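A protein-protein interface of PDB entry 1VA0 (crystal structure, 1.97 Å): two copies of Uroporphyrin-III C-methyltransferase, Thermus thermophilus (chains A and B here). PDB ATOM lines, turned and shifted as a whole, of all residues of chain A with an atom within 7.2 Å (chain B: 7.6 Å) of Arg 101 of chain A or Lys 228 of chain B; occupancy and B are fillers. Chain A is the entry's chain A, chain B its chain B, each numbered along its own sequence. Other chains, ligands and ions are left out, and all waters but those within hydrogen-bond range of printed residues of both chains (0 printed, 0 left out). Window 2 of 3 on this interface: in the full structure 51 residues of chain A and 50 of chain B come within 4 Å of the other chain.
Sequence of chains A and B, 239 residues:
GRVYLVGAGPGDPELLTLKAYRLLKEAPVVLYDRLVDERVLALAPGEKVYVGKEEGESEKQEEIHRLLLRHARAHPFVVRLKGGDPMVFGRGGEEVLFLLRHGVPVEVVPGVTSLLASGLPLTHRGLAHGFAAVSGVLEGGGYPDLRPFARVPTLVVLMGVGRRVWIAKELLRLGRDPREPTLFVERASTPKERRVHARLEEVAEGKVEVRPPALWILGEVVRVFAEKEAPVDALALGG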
ATOM      1  N   GLU A  94     -29.660  16.682 -14.448  1.00  0.00           N
ATOM      2  CA  GLU A  94     -28.937  17.955 -14.434  1.00  0.00           C
ATOM      3  C   GLU A  94     -29.450  18.830 -13.301  1.00  0.00           C
ATOM      4  O   GLU A  94     -28.664  19.484 -12.602  1.00  0.00           O
ATOM      5  CB  GLU A  94     -29.103  18.693 -15.769  1.00  0.00           C
ATOM      6  CG  GLU A  94     -28.433  18.005 -16.949  1.00  0.00           C
ATOM      7  CD  GLU A  94     -28.727  18.714 -18.267  1.00  0.00           C
ATOM      8  OE1 GLU A  94     -28.190  19.815 -18.494  1.00  0.00           O
ATOM      9  OE2 GLU A  94     -29.513  18.174 -19.070  1.00  0.00           O
ATOM     10  N   GLU A  95     -30.768  18.845 -13.111  1.00  0.00           N
ATOM     11  CA  GLU A  95     -31.341  19.660 -12.042  1.00  0.00           C
ATOM     12  C   GLU A  95     -30.839  19.177 -10.687  1.00  0.00           C
ATOM     13  O   GLU A  95     -30.388  19.974  -9.864  1.00  0.00           O
ATOM     14  CB  GLU A  95     -32.873  19.635 -12.120  1.00  0.00           C
ATOM     15  CG  GLU A  95     -33.400  20.254 -13.414  1.00  0.00           C
ATOM     16  CD  GLU A  95     -34.919  20.228 -13.520  1.00  0.00           C
ATOM     17  OE1 GLU A  95     -35.588  19.786 -12.561  1.00  0.00           O
ATOM     18  OE2 GLU A  95     -35.448  20.656 -14.565  1.00  0.00           O
ATOM     19  N   VAL A  96     -30.892  17.870 -10.457  1.00  0.00           N
ATOM     20  CA  VAL A  96     -30.416  17.329  -9.193  1.00  0.00           C
ATOM     21  C   VAL A  96     -28.919  17.617  -8.995  1.00  0.00           C
ATOM     22  O   VAL A  96     -28.492  17.982  -7.899  1.00  0.00           O
ATOM     23  CB  VAL A  96     -30.642  15.794  -9.100  1.00  0.00           C
ATOM     24  CG1 VAL A  96     -29.972  15.243  -7.831  1.00  0.00           C
ATOM     25  CG2 VAL A  96     -32.133  15.484  -9.068  1.00  0.00           C
ATOM     26  N   LEU A  97     -28.130  17.462 -10.054  1.00  0.00           N
ATOM     27  CA  LEU A  97     -26.689  17.692  -9.966  1.00  0.00           C
ATOM     28  C   LEU A  97     -26.377  19.130  -9.552  1.00  0.00           C
ATOM     29  O   LEU A  97     -25.597  19.370  -8.626  1.00  0.00           O
ATOM     30  CB  LEU A  97     -26.032  17.377 -11.309  1.00  0.00           C
ATOM     31  CG  LEU A  97     -24.504  17.434 -11.400  1.00  0.00           C
ATOM     32  CD1 LEU A  97     -23.868  16.683 -10.244  1.00  0.00           C
ATOM     33  CD2 LEU A  97     -24.069  16.838 -12.722  1.00  0.00           C
ATOM     34  N   PHE A  98     -26.999  20.080 -10.242  1.00  0.00           N
ATOM     35  CA  PHE A  98     -26.810  21.495  -9.953  1.00  0.00           C
ATOM     36  C   PHE A  98     -27.141  21.824  -8.504  1.00  0.00           C
ATOM     37  O   PHE A  98     -26.389  22.529  -7.819  1.00  0.00           O
ATOM     38  CB  PHE A  98     -27.691  22.328 -10.894  1.00  0.00           C
ATOM     39  CG  PHE A  98     -27.670  23.796 -10.603  1.00  0.00           C
ATOM     40  CD1 PHE A  98     -28.518  24.341  -9.641  1.00  0.00           C
ATOM     41  CD2 PHE A  98     -26.786  24.636 -11.277  1.00  0.00           C
ATOM     42  CE1 PHE A  98     -28.486  25.711  -9.356  1.00  0.00           C
ATOM     43  CE2 PHE A  98     -26.747  26.005 -10.995  1.00  0.00           C
ATOM     44  CZ  PHE A  98     -27.602  26.539 -10.030  1.00  0.00           C
ATOM     45  N   LEU A  99     -28.272  21.307  -8.034  1.00  0.00           N
ATOM     46  CA  LEU A  99     -28.715  21.567  -6.676  1.00  0.00           C
ATOM     47  C   LEU A  99     -27.757  20.973  -5.651  1.00  0.00           C
ATOM     48  O   LEU A  99     -27.396  21.624  -4.676  1.00  0.00           O
ATOM     49  CB  LEU A  99     -30.139  21.013  -6.486  1.00  0.00           C
ATOM     50  CG  LEU A  99     -31.217  21.773  -7.284  1.00  0.00           C
ATOM     51  CD1 LEU A  99     -32.535  21.024  -7.258  1.00  0.00           C
ATOM     52  CD2 LEU A  99     -31.380  23.169  -6.683  1.00  0.00           C
ATOM     53  N   LEU A 100     -27.337  19.732  -5.866  1.00  0.00           N
ATOM     54  CA  LEU A 100     -26.425  19.105  -4.933  1.00  0.00           C
ATOM     55  C   LEU A 100     -25.132  19.907  -4.882  1.00  0.00           C
ATOM     56  O   LEU A 100     -24.579  20.118  -3.810  1.00  0.00           O
ATOM     57  CB  LEU A 100     -26.153  17.659  -5.334  1.00  0.00           C
ATOM     58  CG  LEU A 100     -27.367  16.737  -5.161  1.00  0.00           C
ATOM     59  CD1 LEU A 100     -26.979  15.328  -5.532  1.00  0.00           C
ATOM     60  CD2 LEU A 100     -27.861  16.765  -3.727  1.00  0.00           C
ATOM     61  N   ARG A 101     -24.672  20.368  -6.040  1.00  0.00           N
ATOM     62  CA  ARG A 101     -23.456  21.167  -6.122  1.00  0.00           C
ATOM     63  C   ARG A 101     -23.593  22.492  -5.369  1.00  0.00           C
ATOM     64  O   ARG A 101     -22.593  23.087  -4.964  1.00  0.00           O
ATOM     65  CB  ARG A 101     -23.092  21.422  -7.588  1.00  0.00           C
ATOM     66  CG  ARG A 101     -22.504  20.191  -8.266  1.00  0.00           C
ATOM     67  CD  ARG A 101     -22.413  20.365  -9.763  1.00  0.00           C
ATOM     68  NE  ARG A 101     -21.519  19.381 -10.365  1.00  0.00           N
ATOM     69  CZ  ARG A 101     -21.259  19.308 -11.667  1.00  0.00           C
ATOM     70  NH1 ARG A 101     -21.830  20.161 -12.511  1.00  0.00           N
ATOM     71  NH2 ARG A 101     -20.424  18.386 -12.127  1.00  0.00           N
ATOM     72  N   HIS A 102     -24.827  22.953  -5.182  1.00  0.00           N
ATOM     73  CA  HIS A 102     -25.056  24.190  -4.447  1.00  0.00           C
ATOM     74  C   HIS A 102     -25.502  23.940  -3.020  1.00  0.00           C
ATOM     75  O   HIS A 102     -26.013  24.833  -2.344  1.00  0.00           O
ATOM     76  CB  HIS A 102     -26.048  25.087  -5.185  1.00  0.00           C
ATOM     77  CG  HIS A 102     -25.450  25.746  -6.387  1.00  0.00           C
ATOM     78  ND1 HIS A 102     -25.256  25.081  -7.579  1.00  0.00           N
ATOM     79  CD2 HIS A 102     -24.918  26.982  -6.553  1.00  0.00           C
ATOM     80  CE1 HIS A 102     -24.628  25.878  -8.427  1.00  0.00           C
ATOM     81  NE2 HIS A 102     -24.411  27.036  -7.830  1.00  0.00           N
ATOM     82  N   GLY A 103     -25.279  22.714  -2.556  1.00  0.00           N
ATOM     83  CA  GLY A 103     -25.627  22.371  -1.191  1.00  0.00           C
ATOM     84  C   GLY A 103     -27.097  22.339  -0.834  1.00  0.00           C
ATOM     85  O   GLY A 103     -27.440  22.485   0.336  1.00  0.00           O
ATOM     86  N   VAL A 104     -27.966  22.163  -1.827  1.00  0.00           N
ATOM     87  CA  VAL A 104     -29.404  22.083  -1.573  1.00  0.00           C
ATOM     88  C   VAL A 104     -29.786  20.608  -1.455  1.00  0.00           C
ATOM     89  O   VAL A 104     -29.502  19.820  -2.357  1.00  0.00           O
ATOM     90  CB  VAL A 104     -30.228  22.689  -2.737  1.00  0.00           C
ATOM     91  CG1 VAL A 104     -31.714  22.470  -2.474  1.00  0.00           C
ATOM     92  CG2 VAL A 104     -29.918  24.168  -2.899  1.00  0.00           C
ATOM     93  N   VAL B 224     -23.171   9.703 -11.849  1.00  0.00           N
ATOM     94  CA  VAL B 224     -23.615  11.086 -12.007  1.00  0.00           C
ATOM     95  C   VAL B 224     -23.593  11.955 -10.739  1.00  0.00           C
ATOM     96  O   VAL B 224     -23.223  13.122 -10.814  1.00  0.00           O
ATOM     97  CB  VAL B 224     -25.043  11.154 -12.649  1.00  0.00           C
ATOM     98  CG1 VAL B 224     -26.093  10.708 -11.656  1.00  0.00           C
ATOM     99  CG2 VAL B 224     -25.334  12.583 -13.132  1.00  0.00           C
ATOM    100  N   PHE B 225     -23.970  11.407  -9.581  1.00  0.00           N
ATOM    101  CA  PHE B 225     -23.992  12.210  -8.350  1.00  0.00           C
ATOM    102  C   PHE B 225     -22.837  11.949  -7.398  1.00  0.00           C
ATOM    103  O   PHE B 225     -22.923  12.263  -6.208  1.00  0.00           O
ATOM    104  CB  PHE B 225     -25.316  12.007  -7.597  1.00  0.00           C
ATOM    105  CG  PHE B 225     -26.538  12.254  -8.441  1.00  0.00           C
ATOM    106  CD1 PHE B 225     -26.661  13.420  -9.195  1.00  0.00           C
ATOM    107  CD2 PHE B 225     -27.563  11.316  -8.489  1.00  0.00           C
ATOM    108  CE1 PHE B 225     -27.793  13.643  -9.993  1.00  0.00           C
ATOM    109  CE2 PHE B 225     -28.701  11.527  -9.280  1.00  0.00           C
ATOM    110  CZ  PHE B 225     -28.818  12.687 -10.033  1.00  0.00           C
ATOM    111  N   ALA B 226     -21.761  11.363  -7.915  1.00  0.00           N
ATOM    112  CA  ALA B 226     -20.592  11.076  -7.093  1.00  0.00           C
ATOM    113  C   ALA B 226     -19.716  12.321  -7.000  1.00  0.00           C
ATOM    114  O   ALA B 226     -19.355  12.911  -8.016  1.00  0.00           O
ATOM    115  CB  ALA B 226     -19.789   9.924  -7.700  1.00  0.00           C
ATOM    116  N   GLU B 227     -19.384  12.722  -5.774  1.00  0.00           N
ATOM    117  CA  GLU B 227     -18.518  13.884  -5.562  1.00  0.00           C
ATOM    118  C   GLU B 227     -17.258  13.708  -6.402  1.00  0.00           C
ATOM    119  O   GLU B 227     -16.864  12.585  -6.708  1.00  0.00           O
ATOM    120  CB  GLU B 227     -18.124  14.011  -4.091  1.00  0.00           C
ATOM    121  CG  GLU B 227     -19.200  14.590  -3.195  1.00  0.00           C
ATOM    122  CD  GLU B 227     -19.371  16.089  -3.370  1.00  0.00           C
ATOM    123  OE1 GLU B 227     -18.761  16.675  -4.297  1.00  0.00           O
ATOM    124  OE2 GLU B 227     -20.128  16.679  -2.570  1.00  0.00           O
ATOM    125  N   LYS B 228     -16.615  14.814  -6.748  1.00  0.00           N
ATOM    126  CA  LYS B 228     -15.420  14.792  -7.582  1.00  0.00           C
ATOM    127  C   LYS B 228     -14.220  14.561  -6.698  1.00  0.00           C
ATOM    128  O   LYS B 228     -13.286  13.796  -7.031  1.00  0.00           O
ATOM    129  CB  LYS B 228     -15.261  16.140  -8.247  1.00  0.00           C
ATOM    130  CG  LYS B 228     -16.564  16.738  -8.685  1.00  0.00           C
ATOM    131  CD  LYS B 228     -16.340  18.130  -9.178  1.00  0.00           C
ATOM    132  CE  LYS B 228     -16.234  18.186 -10.672  1.00  0.00           C
ATOM    133  NZ  LYS B 228     -17.093  19.338 -11.044  1.00  0.00           N
ATOM    134  N   GLU B 229     -14.251  15.260  -5.570  1.00  0.00           N
ATOM    135  CA  GLU B 229     -13.183  15.195  -4.602  1.00  0.00           C
ATOM    136  C   GLU B 229     -13.070  13.903  -3.762  1.00  0.00           C
ATOM    137  O   GLU B 229     -12.093  13.753  -3.018  1.00  0.00           O
ATOM    138  CB  GLU B 229     -13.244  16.482  -3.752  1.00  0.00           C
ATOM    139  CG  GLU B 229     -12.901  17.707  -4.609  1.00  0.00           C
ATOM    140  CD  GLU B 229     -11.485  17.584  -5.127  1.00  0.00           C
ATOM    141  OE1 GLU B 229     -10.675  16.988  -4.385  1.00  0.00           O
ATOM    142  OE2 GLU B 229     -11.171  18.065  -6.241  1.00  0.00           O
ATOM    143  N   ALA B 230     -14.009  12.952  -3.944  1.00  0.00           N
ATOM    144  CA  ALA B 230     -14.023  11.654  -3.197  1.00  0.00           C
ATOM    145  C   ALA B 230     -15.200  10.649  -3.485  1.00  0.00           C
ATOM    146  O   ALA B 230     -16.275  11.068  -3.945  1.00  0.00           O
ATOM    147  CB  ALA B 230     -13.971  11.935  -1.697  1.00  0.00           C
ATOM    148  N   PRO B 231     -15.021   9.315  -3.204  1.00  0.00           N
ATOM    149  CA  PRO B 231     -16.145   8.403  -3.491  1.00  0.00           C
ATOM    150  C   PRO B 231     -17.343   8.587  -2.554  1.00  0.00           C
ATOM    151  O   PRO B 231     -17.715   7.685  -1.785  1.00  0.00           O
ATOM    152  CB  PRO B 231     -15.531   7.013  -3.335  1.00  0.00           C
ATOM    153  CG  PRO B 231     -14.597   7.200  -2.208  1.00  0.00           C
ATOM    154  CD  PRO B 231     -13.922   8.558  -2.559  1.00  0.00           C
ATOM    155  N   VAL B 232     -17.960   9.755  -2.650  1.00  0.00           N
ATOM    156  CA  VAL B 232     -19.096  10.096  -1.812  1.00  0.00           C
ATOM    157  C   VAL B 232     -20.354  10.292  -2.651  1.00  0.00           C
ATOM    158  O   VAL B 232     -20.353  11.055  -3.614  1.00  0.00           O
ATOM    159  CB  VAL B 232     -18.798  11.394  -1.015  1.00  0.00           C
ATOM    160  CG1 VAL B 232     -19.944  11.713  -0.070  1.00  0.00           C
ATOM    161  CG2 VAL B 232     -17.493  11.232  -0.237  1.00  0.00           C
ATOM    162  N   ALA B 234     -23.259  12.052  -3.193  1.00  0.00           N
ATOM    163  CA  ALA B 234     -23.870  13.318  -2.794  1.00  0.00           C
ATOM    164  C   ALA B 234     -25.389  13.263  -2.630  1.00  0.00           C
ATOM    165  O   ALA B 234     -25.939  13.988  -1.803  1.00  0.00           O
ATOM    166  CB  ALA B 234     -23.483  14.427  -3.782  1.00  0.00           C
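N of Ala 234 of chain B sits at hydrogen-bond distance from O of Phe 225 of chain B (3.0 Å).
Among the printed residues, pairs that only touch across the chains: Val 96 of chain A with Phe 225 of chain B, Leu 97 of chain A with Val 224 of chain B, Leu 97 of chain A with Phe 225 of chain B, Leu 100 of chain A with Ala 234 of chain B and Arg 101 of chain A with Lys 228 of chain B.
Of chain B, only Lys 228 comes within 4 Å of Arg 101 of chain A.
Lys 228 of chain B touches just one residue of chain A: Arg 101 (3.6 Å).
Of the printed residues of chain A, Ala 234 of chain B touches Leu 100 (3.9 Å).
Of the printed residues of chain B, Leu 100 of chain A touches Ala 234 (3.9 Å).
Of the printed residues of chain B, Val 96 of chain A touches Phe 225.
Of the printed residues of chain A, Phe 225 of chain B touches Val 96 (3.5 Å) and Leu 97 (3.8 Å).
Of the printed residues of chain A, Val 224 of chain B touches Leu 97 (3.7 Å).
Gly 103 of chain A touches none of the printed residues of chain B.
His 102 of chain A touches none of the printed residues of chain B.
The nearest residue of chain B that does not touch Arg 101 of chain A is Val 224 of chain B (6.1 Å).
The nearest printed residue of chain A that does not touch Ala 234 of chain B is Arg 101 of chain A (6.5 Å).
Of the 10 printed residues of chain B, 4 touch a printed residue of chain A.
Hydrophobic or aromatic side chains of chain B within 4 Å of the printed part of chain A: Phe 225.
Of the 11 printed residues of chain A, 4 touch a printed residue of chain B.
Along chain A the printed residues that touch a printed residue of chain B span positions 96 to 101.
Among the printed residues, no Asp or Glu carboxylate lies within 4 Å of a Lys or Arg side-chain nitrogen of the other chain.
No position is printed for both chains.
Of the 5 pairs that touch across the chains among the printed residues, none has its exchanged pair printed and touching as well.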
